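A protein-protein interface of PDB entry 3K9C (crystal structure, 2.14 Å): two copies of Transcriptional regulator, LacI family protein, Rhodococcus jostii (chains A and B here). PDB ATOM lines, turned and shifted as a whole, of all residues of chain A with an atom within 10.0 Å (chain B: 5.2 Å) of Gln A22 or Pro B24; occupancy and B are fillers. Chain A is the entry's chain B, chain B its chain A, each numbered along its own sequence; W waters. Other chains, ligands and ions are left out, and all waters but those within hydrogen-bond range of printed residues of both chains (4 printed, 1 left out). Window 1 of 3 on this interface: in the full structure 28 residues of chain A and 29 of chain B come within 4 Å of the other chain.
OE1 of Gln B22 is in hydrogen-bond range of NE of Arg A224 (3.4 Å). The guanidinium group (NH1) of Arg A224 sits close to the guanidinium group (NH2) of Arg B195, at 3.2 Å. The guanidinium group of Arg B224 lies close to the guanidinium group of Arg A195 (3.3 Å). The side-chain hydroxyl (OG) of Ser A52 lies within hydrogen-bond range of the side-chain carboxylate (OE2) of Glu B31, at 2.7 Å. NH2 of Arg B224 is in salt-bridge range of OE1 of Glu A169 (2.6 Å). NE2 of Gln A22 lies within hydrogen-bond range of OD1 of Asp B28, at 3.3 Å.
OD1 of Asn A193 sits at hydrogen-bond distance from N of Arg A195, at 3.2 Å. The side-chain carboxylate (OE2) of Glu A169 is in salt-bridge range of the guanidinium group (NE) of Arg A195 (3.5 Å). The guanidinium group (NH1) of Arg B195 sits at hydrogen-bond distance from the backbone carbonyl oxygen (O) of Gln B22, 2.6 Å away. O of Gln A22 is in hydrogen-bond range of NH2 of Arg A195, 2.7 Å away. The backbone NH (N) of Leu A21 is in hydrogen-bond range of the backbone carbonyl oxygen (O) of Val A49.
Among the printed residues, merely in contact across the chains: Gln A22 with Arg B224 (3.1 Å), Leu A21 with Gly B27 (3.2 Å), Pro A51 with Glu B31 (3.6 Å), Ala A50 with Glu B31 (3.6 Å), Gln A22 with Gly B27 (3.7 Å), Gln A22 with Pro B24 (3.7 Å) and Leu A21 with Glu B31 (3.8 Å).
Gln A22 touches just these residues of chain B: Pro B24 (3.7 Å), Gly B27 (3.7 Å), Asp B28 (3.3 Å) and Arg B224 (3.1 Å). Of the printed residues of chain B, Pro A51 touches Glu B31 (3.6 Å). Printed residues of chain B within 4 Å of Arg A224: Gln B22 (3.4 Å) and Arg B195 (3.2 Å). No residue of chain A comes within 4 Å of Gln B23. Gly B27 touches two residues of chain A. Of the printed residues of chain A, Arg B195 touches Arg A224. The nearest printed residue of chain A that does not touch Asp B28 is Leu A21 (5.2 Å).
Hydrophobic or aromatic side chains of chain A within 4 Å of the printed part of chain B: Leu A21, Ala A50 and Pro A51. Of the 12 printed residues of chain B, 7 touch a printed residue of chain A. Along chain B the printed residues that touch a printed residue of chain A span positions 22 to 224. Among the printed residues, 13 pairs touch across the chains.
Gln A22 touches Pro B24, but with the chains exchanged Pro A24 does not touch Gln B22 (7.1 Å). Gln A22 touches Gly B27, but with the chains exchanged Gly A27 does not touch Gln B22 (6.4 Å). Gln A22 touches Asp B28, but with the chains exchanged Asp A28 does not touch Gln B22 (5.5 Å). Arg A195 touches Arg B224, and with the chains exchanged Arg A224 touches Arg B195. Of the 13 pairs that touch across the chains among the printed residues, 4 have their exchanged pair printed and touching as well.
Water W4 bridges the side-chain carboxylate of Glu B31 (2.5 Å) and the side-chain amide nitrogen of Gln A22 (2.9 Å). Water W1 lies within hydrogen-bond range of the guanidinium group (NH1) of Arg B224 and the guanidinium group (NH2) of Arg A195. Water W2 bridges OG of Ser A52 (2.8 Å) and O of Glu B31 (2.9 Å). Water W3 bridges O of Gly A27 (3.3 Å) and NE2 of Gln B22 (3.5 Å).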
ATOM      1  N   PHE A  19      15.035  29.834  16.715  1.00  0.00           N
ATOM      2  CA  PHE A  19      14.008  29.178  17.541  1.00  0.00           C
ATOM      3  C   PHE A  19      13.067  30.176  18.210  1.00  0.00           C
ATOM      4  O   PHE A  19      13.405  31.349  18.377  1.00  0.00           O
ATOM      5  CB  PHE A  19      14.664  28.327  18.637  1.00  0.00           C
ATOM      6  CG  PHE A  19      15.136  29.126  19.811  1.00  0.00           C
ATOM      7  CD1 PHE A  19      14.456  29.074  21.021  1.00  0.00           C
ATOM      8  CD2 PHE A  19      16.247  29.952  19.701  1.00  0.00           C
ATOM      9  CE1 PHE A  19      14.878  29.835  22.109  1.00  0.00           C
ATOM     10  CE2 PHE A  19      16.677  30.715  20.774  1.00  0.00           C
ATOM     11  CZ  PHE A  19      15.995  30.657  21.981  1.00  0.00           C
ATOM     12  N   GLU A  20      11.891  29.695  18.609  1.00  0.00           N
ATOM     13  CA  GLU A  20      10.897  30.540  19.267  1.00  0.00           C
ATOM     14  C   GLU A  20      11.126  30.658  20.767  1.00  0.00           C
ATOM     15  O   GLU A  20      11.056  29.666  21.502  1.00  0.00           O
ATOM     16  CB  GLU A  20       9.488  29.995  19.033  1.00  0.00           C
ATOM     17  CG  GLU A  20       8.938  30.245  17.653  1.00  0.00           C
ATOM     18  CD  GLU A  20       7.610  29.545  17.427  1.00  0.00           C
ATOM     19  OE1 GLU A  20       6.721  29.631  18.310  1.00  0.00           O
ATOM     20  OE2 GLU A  20       7.456  28.911  16.364  1.00  0.00           O
ATOM     21  N   LEU A  21      11.395  31.879  21.213  1.00  0.00           N
ATOM     22  CA  LEU A  21      11.613  32.148  22.627  1.00  0.00           C
ATOM     23  C   LEU A  21      10.383  31.692  23.429  1.00  0.00           C
ATOM     24  O   LEU A  21       9.242  31.883  23.008  1.00  0.00           O
ATOM     25  CB  LEU A  21      11.848  33.646  22.837  1.00  0.00           C
ATOM     26  CG  LEU A  21      12.729  34.055  24.021  1.00  0.00           C
ATOM     27  CD1 LEU A  21      14.097  33.415  23.876  1.00  0.00           C
ATOM     28  CD2 LEU A  21      12.862  35.576  24.076  1.00  0.00           C
ATOM     29  N   GLN A  22      10.618  31.077  24.579  1.00  0.00           N
ATOM     30  CA  GLN A  22       9.521  30.619  25.425  1.00  0.00           C
ATOM     31  C   GLN A  22       8.607  29.550  24.803  1.00  0.00           C
ATOM     32  O   GLN A  22       7.436  29.455  25.161  1.00  0.00           O
ATOM     33  CB  GLN A  22       8.665  31.811  25.867  1.00  0.00           C
ATOM     34  CG  GLN A  22       9.460  32.927  26.513  1.00  0.00           C
ATOM     35  CD  GLN A  22       8.586  33.879  27.297  1.00  0.00           C
ATOM     36  OE1 GLN A  22       7.895  33.467  28.229  1.00  0.00           O
ATOM     37  NE2 GLN A  22       8.613  35.160  26.930  1.00  0.00           N
ATOM     38  N   GLN A  23       9.124  28.768  23.862  1.00  0.00           N
ATOM     39  CA  GLN A  23       8.329  27.694  23.275  1.00  0.00           C
ATOM     40  C   GLN A  23       8.934  26.439  23.893  1.00  0.00           C
ATOM     41  O   GLN A  23      10.061  26.078  23.593  1.00  0.00           O
ATOM     42  CB  GLN A  23       8.473  27.659  21.754  1.00  0.00           C
ATOM     43  CG  GLN A  23       7.502  26.713  21.079  1.00  0.00           C
ATOM     44  CD  GLN A  23       6.056  27.157  21.252  1.00  0.00           C
ATOM     45  OE1 GLN A  23       5.674  28.244  20.812  1.00  0.00           O
ATOM     46  NE2 GLN A  23       5.246  26.319  21.897  1.00  0.00           N
ATOM     47  N   PRO A  24       8.189  25.765  24.776  1.00  0.00           N
ATOM     48  CA  PRO A  24       8.661  24.550  25.452  1.00  0.00           C
ATOM     49  C   PRO A  24       9.461  23.568  24.596  1.00  0.00           C
ATOM     50  O   PRO A  24      10.608  23.252  24.919  1.00  0.00           O
ATOM     51  CB  PRO A  24       7.371  23.941  25.997  1.00  0.00           C
ATOM     52  CG  PRO A  24       6.559  25.172  26.320  1.00  0.00           C
ATOM     53  CD  PRO A  24       6.768  26.007  25.078  1.00  0.00           C
ATOM     54  N   PHE A  25       8.861  23.095  23.510  1.00  0.00           N
ATOM     55  CA  PHE A  25       9.533  22.143  22.636  1.00  0.00           C
ATOM     56  C   PHE A  25      10.808  22.688  21.983  1.00  0.00           C
ATOM     57  O   PHE A  25      11.738  21.930  21.746  1.00  0.00           O
ATOM     58  CB  PHE A  25       8.573  21.630  21.561  1.00  0.00           C
ATOM     59  CG  PHE A  25       9.143  20.516  20.728  1.00  0.00           C
ATOM     60  CD1 PHE A  25       9.633  19.358  21.334  1.00  0.00           C
ATOM     61  CD2 PHE A  25       9.205  20.626  19.347  1.00  0.00           C
ATOM     62  CE1 PHE A  25      10.180  18.327  20.569  1.00  0.00           C
ATOM     63  CE2 PHE A  25       9.746  19.609  18.576  1.00  0.00           C
ATOM     64  CZ  PHE A  25      10.236  18.454  19.187  1.00  0.00           C
ATOM     65  N   HIS A  26      10.856  23.986  21.679  1.00  0.00           N
ATOM     66  CA  HIS A  26      12.075  24.545  21.083  1.00  0.00           C
ATOM     67  C   HIS A  26      13.160  24.608  22.148  1.00  0.00           C
ATOM     68  O   HIS A  26      14.347  24.471  21.845  1.00  0.00           O
ATOM     69  CB  HIS A  26      11.839  25.941  20.504  1.00  0.00           C
ATOM     70  CG  HIS A  26      10.982  25.950  19.280  1.00  0.00           C
ATOM     71  ND1 HIS A  26      10.939  27.020  18.412  1.00  0.00           N
ATOM     72  CD2 HIS A  26      10.106  25.037  18.795  1.00  0.00           C
ATOM     73  CE1 HIS A  26      10.069  26.770  17.449  1.00  0.00           C
ATOM     74  NE2 HIS A  26       9.549  25.573  17.659  1.00  0.00           N
ATOM     75  N   GLY A  27      12.749  24.826  23.395  1.00  0.00           N
ATOM     76  CA  GLY A  27      13.707  24.843  24.487  1.00  0.00           C
ATOM     77  C   GLY A  27      14.397  23.484  24.618  1.00  0.00           C
ATOM     78  O   GLY A  27      15.618  23.415  24.770  1.00  0.00           O
ATOM     79  N   ASP A  28      13.624  22.398  24.558  1.00  0.00           N
ATOM     80  CA  ASP A  28      14.197  21.047  24.652  1.00  0.00           C
ATOM     81  C   ASP A  28      15.146  20.779  23.485  1.00  0.00           C
ATOM     82  O   ASP A  28      16.233  20.238  23.668  1.00  0.00           O
ATOM     83  CB  ASP A  28      13.107  19.971  24.620  1.00  0.00           C
ATOM     84  CG  ASP A  28      12.195  20.016  25.827  1.00  0.00           C
ATOM     85  OD1 ASP A  28      12.697  20.098  26.969  1.00  0.00           O
ATOM     86  OD2 ASP A  28      10.962  19.951  25.628  1.00  0.00           O
ATOM     87  N   VAL A  30      16.706  23.008  21.592  1.00  0.00           N
ATOM     88  CA  VAL A  30      17.903  23.846  21.687  1.00  0.00           C
ATOM     89  C   VAL A  30      18.916  23.244  22.661  1.00  0.00           C
ATOM     90  O   VAL A  30      20.102  23.143  22.346  1.00  0.00           O
ATOM     91  CB  VAL A  30      17.571  25.285  22.160  1.00  0.00           C
ATOM     92  CG1 VAL A  30      18.841  25.973  22.641  1.00  0.00           C
ATOM     93  CG2 VAL A  30      16.943  26.090  21.010  1.00  0.00           C
ATOM     94  N   ALA A  48      16.834  34.357  18.312  1.00  0.00           N
ATOM     95  CA  ALA A  48      15.464  34.117  18.734  1.00  0.00           C
ATOM     96  C   ALA A  48      14.354  34.830  17.981  1.00  0.00           C
ATOM     97  O   ALA A  48      14.508  35.964  17.525  1.00  0.00           O
ATOM     98  CB  ALA A  48      15.336  34.420  20.224  1.00  0.00           C
ATOM     99  N   VAL A  49      13.228  34.139  17.858  1.00  0.00           N
ATOM    100  CA  VAL A  49      12.043  34.689  17.228  1.00  0.00           C
ATOM    101  C   VAL A  49      11.074  34.948  18.390  1.00  0.00           C
ATOM    102  O   VAL A  49      10.946  34.111  19.292  1.00  0.00           O
ATOM    103  CB  VAL A  49      11.404  33.684  16.227  1.00  0.00           C
ATOM    104  CG1 VAL A  49      10.075  34.232  15.707  1.00  0.00           C
ATOM    105  CG2 VAL A  49      12.360  33.422  15.066  1.00  0.00           C
ATOM    106  N   ALA A  50      10.425  36.114  18.374  1.00  0.00           N
ATOM    107  CA  ALA A  50       9.458  36.503  19.401  1.00  0.00           C
ATOM    108  C   ALA A  50       8.448  37.460  18.774  1.00  0.00           C
ATOM    109  O   ALA A  50       8.668  37.955  17.672  1.00  0.00           O
ATOM    110  CB  ALA A  50      10.165  37.175  20.560  1.00  0.00           C
ATOM    111  N   PRO A  51       7.330  37.742  19.471  1.00  0.00           N
ATOM    112  CA  PRO A  51       6.326  38.652  18.905  1.00  0.00           C
ATOM    113  C   PRO A  51       6.910  39.945  18.347  1.00  0.00           C
ATOM    114  O   PRO A  51       6.504  40.395  17.281  1.00  0.00           O
ATOM    115  CB  PRO A  51       5.377  38.898  20.078  1.00  0.00           C
ATOM    116  CG  PRO A  51       5.432  37.590  20.819  1.00  0.00           C
ATOM    117  CD  PRO A  51       6.921  37.283  20.810  1.00  0.00           C
ATOM    118  N   SER A  52       7.864  40.538  19.058  1.00  0.00           N
ATOM    119  CA  SER A  52       8.463  41.779  18.584  1.00  0.00           C
ATOM    120  C   SER A  52       9.721  41.550  17.759  1.00  0.00           C
ATOM    121  O   SER A  52      10.448  42.493  17.468  1.00  0.00           O
ATOM    122  CB  SER A  52       8.778  42.717  19.760  1.00  0.00           C
ATOM    123  OG  SER A  52       9.784  42.192  20.607  1.00  0.00           O
ATOM    124  N   THR A 167      -1.264  26.613  19.582  1.00  0.00           N
ATOM    125  CA  THR A 167      -0.136  26.063  20.329  1.00  0.00           C
ATOM    126  C   THR A 167      -0.036  26.555  21.768  1.00  0.00           C
ATOM    127  O   THR A 167       0.886  26.172  22.482  1.00  0.00           O
ATOM    128  CB  THR A 167       1.200  26.423  19.649  1.00  0.00           C
ATOM    129  OG1 THR A 167       1.377  27.847  19.690  1.00  0.00           O
ATOM    130  CG2 THR A 167       1.209  25.967  18.197  1.00  0.00           C
ATOM    131  N   THR A 168      -0.966  27.402  22.196  1.00  0.00           N
ATOM    132  CA  THR A 168      -0.896  27.937  23.553  1.00  0.00           C
ATOM    133  C   THR A 168      -2.003  27.421  24.459  1.00  0.00           C
ATOM    134  O   THR A 168      -2.987  26.834  23.994  1.00  0.00           O
ATOM    135  CB  THR A 168      -0.968  29.473  23.557  1.00  0.00           C
ATOM    136  OG1 THR A 168      -2.319  29.880  23.301  1.00  0.00           O
ATOM    137  CG2 THR A 168      -0.055  30.057  22.481  1.00  0.00           C
ATOM    138  N   GLU A 169      -1.837  27.657  25.759  1.00  0.00           N
ATOM    139  CA  GLU A 169      -2.816  27.217  26.747  1.00  0.00           C
ATOM    140  C   GLU A 169      -4.201  27.809  26.499  1.00  0.00           C
ATOM    141  O   GLU A 169      -5.210  27.174  26.794  1.00  0.00           O
ATOM    142  CB  GLU A 169      -2.351  27.572  28.170  1.00  0.00           C
ATOM    143  CG  GLU A 169      -0.954  27.062  28.529  1.00  0.00           C
ATOM    144  CD  GLU A 169       0.159  28.049  28.187  1.00  0.00           C
ATOM    145  OE1 GLU A 169      -0.012  28.857  27.255  1.00  0.00           O
ATOM    146  OE2 GLU A 169       1.217  28.014  28.850  1.00  0.00           O
ATOM    147  N   ASN A 193      -0.492  20.091  21.158  1.00  0.00           N
ATOM    148  CA  ASN A 193       0.773  19.935  21.875  1.00  0.00           C
ATOM    149  C   ASN A 193       0.559  20.042  23.389  1.00  0.00           C
ATOM    150  O   ASN A 193      -0.545  20.346  23.843  1.00  0.00           O
ATOM    151  CB  ASN A 193       1.834  20.953  21.381  1.00  0.00           C
ATOM    152  CG  ASN A 193       1.534  22.410  21.775  1.00  0.00           C
ATOM    153  OD1 ASN A 193       0.618  22.708  22.535  1.00  0.00           O
ATOM    154  ND2 ASN A 193       2.340  23.320  21.255  1.00  0.00           N
ATOM    155  N   ARG A 195       1.495  22.280  25.612  1.00  0.00           N
ATOM    156  CA  ARG A 195       1.069  23.589  26.106  1.00  0.00           C
ATOM    157  C   ARG A 195      -0.429  23.764  25.898  1.00  0.00           C
ATOM    158  O   ARG A 195      -1.122  24.351  26.729  1.00  0.00           O
ATOM    159  CB  ARG A 195       1.838  24.714  25.405  1.00  0.00           C
ATOM    160  CG  ARG A 195       1.458  26.098  25.905  1.00  0.00           C
ATOM    161  CD  ARG A 195       2.366  27.165  25.332  1.00  0.00           C
ATOM    162  NE  ARG A 195       3.494  27.440  26.212  1.00  0.00           N
ATOM    163  CZ  ARG A 195       4.486  28.274  25.914  1.00  0.00           C
ATOM    164  NH1 ARG A 195       4.490  28.913  24.748  1.00  0.00           N
ATOM    165  NH2 ARG A 195       5.467  28.482  26.786  1.00  0.00           N
ATOM    166  N   SER A 223       7.252  17.498  26.560  1.00  0.00           N
ATOM    167  CA  SER A 223       8.072  18.616  26.999  1.00  0.00           C
ATOM    168  C   SER A 223       8.033  18.687  28.522  1.00  0.00           C
ATOM    169  O   SER A 223       7.330  17.903  29.158  1.00  0.00           O
ATOM    170  CB  SER A 223       7.552  19.921  26.382  1.00  0.00           C
ATOM    171  OG  SER A 223       6.288  20.272  26.907  1.00  0.00           O
ATOM    172  N   ARG A 224       8.782  19.626  29.097  1.00  0.00           N
ATOM    173  CA  ARG A 224       8.854  19.777  30.549  1.00  0.00           C
ATOM    174  C   ARG A 224       7.485  19.920  31.201  1.00  0.00           C
ATOM    175  O   ARG A 224       7.294  19.540  32.354  1.00  0.00           O
ATOM    176  CB  ARG A 224       9.720  20.990  30.927  1.00  0.00           C
ATOM    177  CG  ARG A 224       9.116  22.347  30.578  1.00  0.00           C
ATOM    178  CD  ARG A 224       9.965  23.494  31.128  1.00  0.00           C
ATOM    179  NE  ARG A 224      10.037  23.481  32.588  1.00  0.00           N
ATOM    180  CZ  ARG A 224       9.057  23.875  33.392  1.00  0.00           C
ATOM    181  NH1 ARG A 224       7.918  24.328  32.881  1.00  0.00           N
ATOM    182  NH2 ARG A 224       9.211  23.806  34.710  1.00  0.00           N
ATOM    183  N   LEU A 225       6.532  20.466  30.460  1.00  0.00           N
ATOM    184  CA  LEU A 225       5.185  20.660  30.983  1.00  0.00           C
ATOM    185  C   LEU A 225       4.557  19.323  31.364  1.00  0.00           C
ATOM    186  O   LEU A 225       3.940  19.198  32.412  1.00  0.00           O
ATOM    187  CB  LEU A 225       4.311  21.339  29.921  1.00  0.00           C
ATOM    188  CG  LEU A 225       4.800  22.673  29.349  1.00  0.00           C
ATOM    189  CD1 LEU A 225       3.943  23.069  28.166  1.00  0.00           C
ATOM    190  CD2 LEU A 225       4.750  23.736  30.434  1.00  0.00           C
ATOM    191  N   GLN B  22      14.616  27.780  30.082  1.00  0.00           N
ATOM    192  CA  GLN B  22      13.224  27.543  30.467  1.00  0.00           C
ATOM    193  C   GLN B  22      12.647  28.514  31.493  1.00  0.00           C
ATOM    194  O   GLN B  22      11.763  28.149  32.261  1.00  0.00           O
ATOM    195  CB  GLN B  22      13.050  26.095  30.961  1.00  0.00           C
ATOM    196  CG  GLN B  22      14.305  25.449  31.553  1.00  0.00           C
ATOM    197  CD  GLN B  22      14.083  23.996  31.953  1.00  0.00           C
ATOM    198  OE1 GLN B  22      13.422  23.708  32.953  1.00  0.00           O
ATOM    199  NE2 GLN B  22      14.623  23.074  31.164  1.00  0.00           N
ATOM    200  N   GLN B  23      13.118  29.756  31.489  1.00  0.00           N
ATOM    201  CA  GLN B  23      12.641  30.731  32.458  1.00  0.00           C
ATOM    202  C   GLN B  23      11.844  31.867  31.804  1.00  0.00           C
ATOM    203  O   GLN B  23      12.403  32.698  31.099  1.00  0.00           O
ATOM    204  CB  GLN B  23      13.839  31.286  33.238  1.00  0.00           C
ATOM    205  CG  GLN B  23      13.484  31.966  34.545  1.00  0.00           C
ATOM    206  CD  GLN B  23      12.609  31.094  35.432  1.00  0.00           C
ATOM    207  OE1 GLN B  23      13.002  29.994  35.829  1.00  0.00           O
ATOM    208  NE2 GLN B  23      11.411  31.581  35.739  1.00  0.00           N
ATOM    209  N   PRO B  24      10.520  31.911  32.040  1.00  0.00           N
ATOM    210  CA  PRO B  24       9.619  32.933  31.485  1.00  0.00           C
ATOM    211  C   PRO B  24      10.131  34.368  31.643  1.00  0.00           C
ATOM    212  O   PRO B  24      10.098  35.140  30.694  1.00  0.00           O
ATOM    213  CB  PRO B  24       8.324  32.710  32.253  1.00  0.00           C
ATOM    214  CG  PRO B  24       8.375  31.247  32.581  1.00  0.00           C
ATOM    215  CD  PRO B  24       9.800  31.054  33.000  1.00  0.00           C
ATOM    216  N   PHE B  25      10.604  34.720  32.838  1.00  0.00           N
ATOM    217  CA  PHE B  25      11.111  36.075  33.079  1.00  0.00           C
ATOM    218  C   PHE B  25      12.329  36.379  32.210  1.00  0.00           C
ATOM    219  O   PHE B  25      12.480  37.499  31.716  1.00  0.00           O
ATOM    220  CB  PHE B  25      11.468  36.278  34.555  1.00  0.00           C
ATOM    221  CG  PHE B  25      11.898  37.686  34.885  1.00  0.00           C
ATOM    222  CD1 PHE B  25      11.158  38.780  34.435  1.00  0.00           C
ATOM    223  CD2 PHE B  25      13.035  37.919  35.649  1.00  0.00           C
ATOM    224  CE1 PHE B  25      11.546  40.081  34.740  1.00  0.00           C
ATOM    225  CE2 PHE B  25      13.430  39.218  35.957  1.00  0.00           C
ATOM    226  CZ  PHE B  25      12.685  40.298  35.501  1.00  0.00           C
ATOM    227  N   HIS B  26      13.202  35.394  32.023  1.00  0.00           N
ATOM    228  CA  HIS B  26      14.367  35.624  31.169  1.00  0.00           C
ATOM    229  C   HIS B  26      13.915  35.764  29.724  1.00  0.00           C
ATOM    230  O   HIS B  26      14.547  36.459  28.927  1.00  0.00           O
ATOM    231  CB  HIS B  26      15.382  34.488  31.298  1.00  0.00           C
ATOM    232  CG  HIS B  26      16.104  34.478  32.608  1.00  0.00           C
ATOM    233  ND1 HIS B  26      17.162  33.635  32.866  1.00  0.00           N
ATOM    234  CD2 HIS B  26      15.907  35.200  33.736  1.00  0.00           C
ATOM    235  CE1 HIS B  26      17.586  33.837  34.101  1.00  0.00           C
ATOM    236  NE2 HIS B  26      16.842  34.782  34.651  1.00  0.00           N
ATOM    237  N   GLY B  27      12.816  35.096  29.391  1.00  0.00           N
ATOM    238  CA  GLY B  27      12.279  35.183  28.045  1.00  0.00           C
ATOM    239  C   GLY B  27      11.878  36.627  27.772  1.00  0.00           C
ATOM    240  O   GLY B  27      12.216  37.193  26.725  1.00  0.00           O
ATOM    241  N   ASP B  28      11.161  37.237  28.715  1.00  0.00           N
ATOM    242  CA  ASP B  28      10.753  38.622  28.535  1.00  0.00           C
ATOM    243  C   ASP B  28      11.983  39.519  28.466  1.00  0.00           C
ATOM    244  O   ASP B  28      12.102  40.349  27.572  1.00  0.00           O
ATOM    245  CB  ASP B  28       9.835  39.078  29.674  1.00  0.00           C
ATOM    246  CG  ASP B  28       8.514  38.332  29.688  1.00  0.00           C
ATOM    247  OD1 ASP B  28       8.051  37.935  28.599  1.00  0.00           O
ATOM    248  OD2 ASP B  28       7.936  38.152  30.779  1.00  0.00           O
ATOM    249  N   GLU B  31      13.814  39.123  25.012  1.00  0.00           N
ATOM    250  CA  GLU B  31      13.084  39.774  23.936  1.00  0.00           C
ATOM    251  C   GLU B  31      13.302  41.287  24.013  1.00  0.00           C
ATOM    252  O   GLU B  31      13.530  41.939  23.000  1.00  0.00           O
ATOM    253  CB  GLU B  31      11.580  39.460  24.025  1.00  0.00           C
ATOM    254  CG  GLU B  31      10.749  40.171  22.963  1.00  0.00           C
ATOM    255  CD  GLU B  31       9.286  39.741  22.944  1.00  0.00           C
ATOM    256  OE1 GLU B  31       8.881  38.922  23.800  1.00  0.00           O
ATOM    257  OE2 GLU B  31       8.543  40.234  22.066  1.00  0.00           O
ATOM    258  N   ARG B 195       5.847  31.218  37.915  1.00  0.00           N
ATOM    259  CA  ARG B 195       5.895  29.772  37.697  1.00  0.00           C
ATOM    260  C   ARG B 195       5.577  29.079  39.013  1.00  0.00           C
ATOM    261  O   ARG B 195       4.808  28.123  39.055  1.00  0.00           O
ATOM    262  CB  ARG B 195       7.269  29.337  37.190  1.00  0.00           C
ATOM    263  CG  ARG B 195       7.463  27.834  37.180  1.00  0.00           C
ATOM    264  CD  ARG B 195       8.730  27.453  36.449  1.00  0.00           C
ATOM    265  NE  ARG B 195       8.518  27.423  35.009  1.00  0.00           N
ATOM    266  CZ  ARG B 195       9.495  27.316  34.116  1.00  0.00           C
ATOM    267  NH1 ARG B 195      10.755  27.239  34.531  1.00  0.00           N
ATOM    268  NH2 ARG B 195       9.212  27.274  32.816  1.00  0.00           N
ATOM    269  N   SER B 223       4.913  37.555  33.985  1.00  0.00           N
ATOM    270  CA  SER B 223       5.373  36.801  32.824  1.00  0.00           C
ATOM    271  C   SER B 223       4.169  36.342  31.998  1.00  0.00           C
ATOM    272  O   SER B 223       3.018  36.629  32.344  1.00  0.00           O
ATOM    273  CB  SER B 223       6.165  35.574  33.286  1.00  0.00           C
ATOM    274  OG  SER B 223       5.307  34.645  33.926  1.00  0.00           O
ATOM    275  N   ARG B 224       4.433  35.627  30.909  1.00  0.00           N
ATOM    276  CA  ARG B 224       3.356  35.149  30.050  1.00  0.00           C
ATOM    277  C   ARG B 224       2.386  34.265  30.819  1.00  0.00           C
ATOM    278  O   ARG B 224       1.225  34.151  30.454  1.00  0.00           O
ATOM    279  CB  ARG B 224       3.916  34.376  28.847  1.00  0.00           C
ATOM    280  CG  ARG B 224       4.679  33.091  29.190  1.00  0.00           C
ATOM    281  CD  ARG B 224       5.018  32.314  27.910  1.00  0.00           C
ATOM    282  NE  ARG B 224       3.799  31.903  27.212  1.00  0.00           N
ATOM    283  CZ  ARG B 224       3.023  30.887  27.588  1.00  0.00           C
ATOM    284  NH1 ARG B 224       3.336  30.160  28.650  1.00  0.00           N
ATOM    285  NH2 ARG B 224       1.909  30.614  26.917  1.00  0.00           N
ATOM    286  N   LEU B 225       2.864  33.647  31.893  1.00  0.00           N
ATOM    287  CA  LEU B 225       2.024  32.773  32.699  1.00  0.00           C
ATOM    288  C   LEU B 225       0.907  33.529  33.431  1.00  0.00           C
ATOM    289  O   LEU B 225      -0.222  33.046  33.524  1.00  0.00           O
ATOM    290  CB  LEU B 225       2.880  32.013  33.719  1.00  0.00           C
ATOM    291  CG  LEU B 225       3.948  31.044  33.204  1.00  0.00           C
ATOM    292  CD1 LEU B 225       4.798  30.565  34.373  1.00  0.00           C
ATOM    293  CD2 LEU B 225       3.291  29.858  32.488  1.00  0.00           C
HETATM  294  O   HOH W   1       5.773  29.695  29.558  1.00  0.00           O
HETATM  295  O   HOH W   2      12.578  41.985  20.289  1.00  0.00           O
HETATM  296  O   HOH W   3      16.003  23.336  28.008  1.00  0.00           O
HETATM  297  O   HOH W   4       9.322  36.568  24.540  1.00  0.00           O
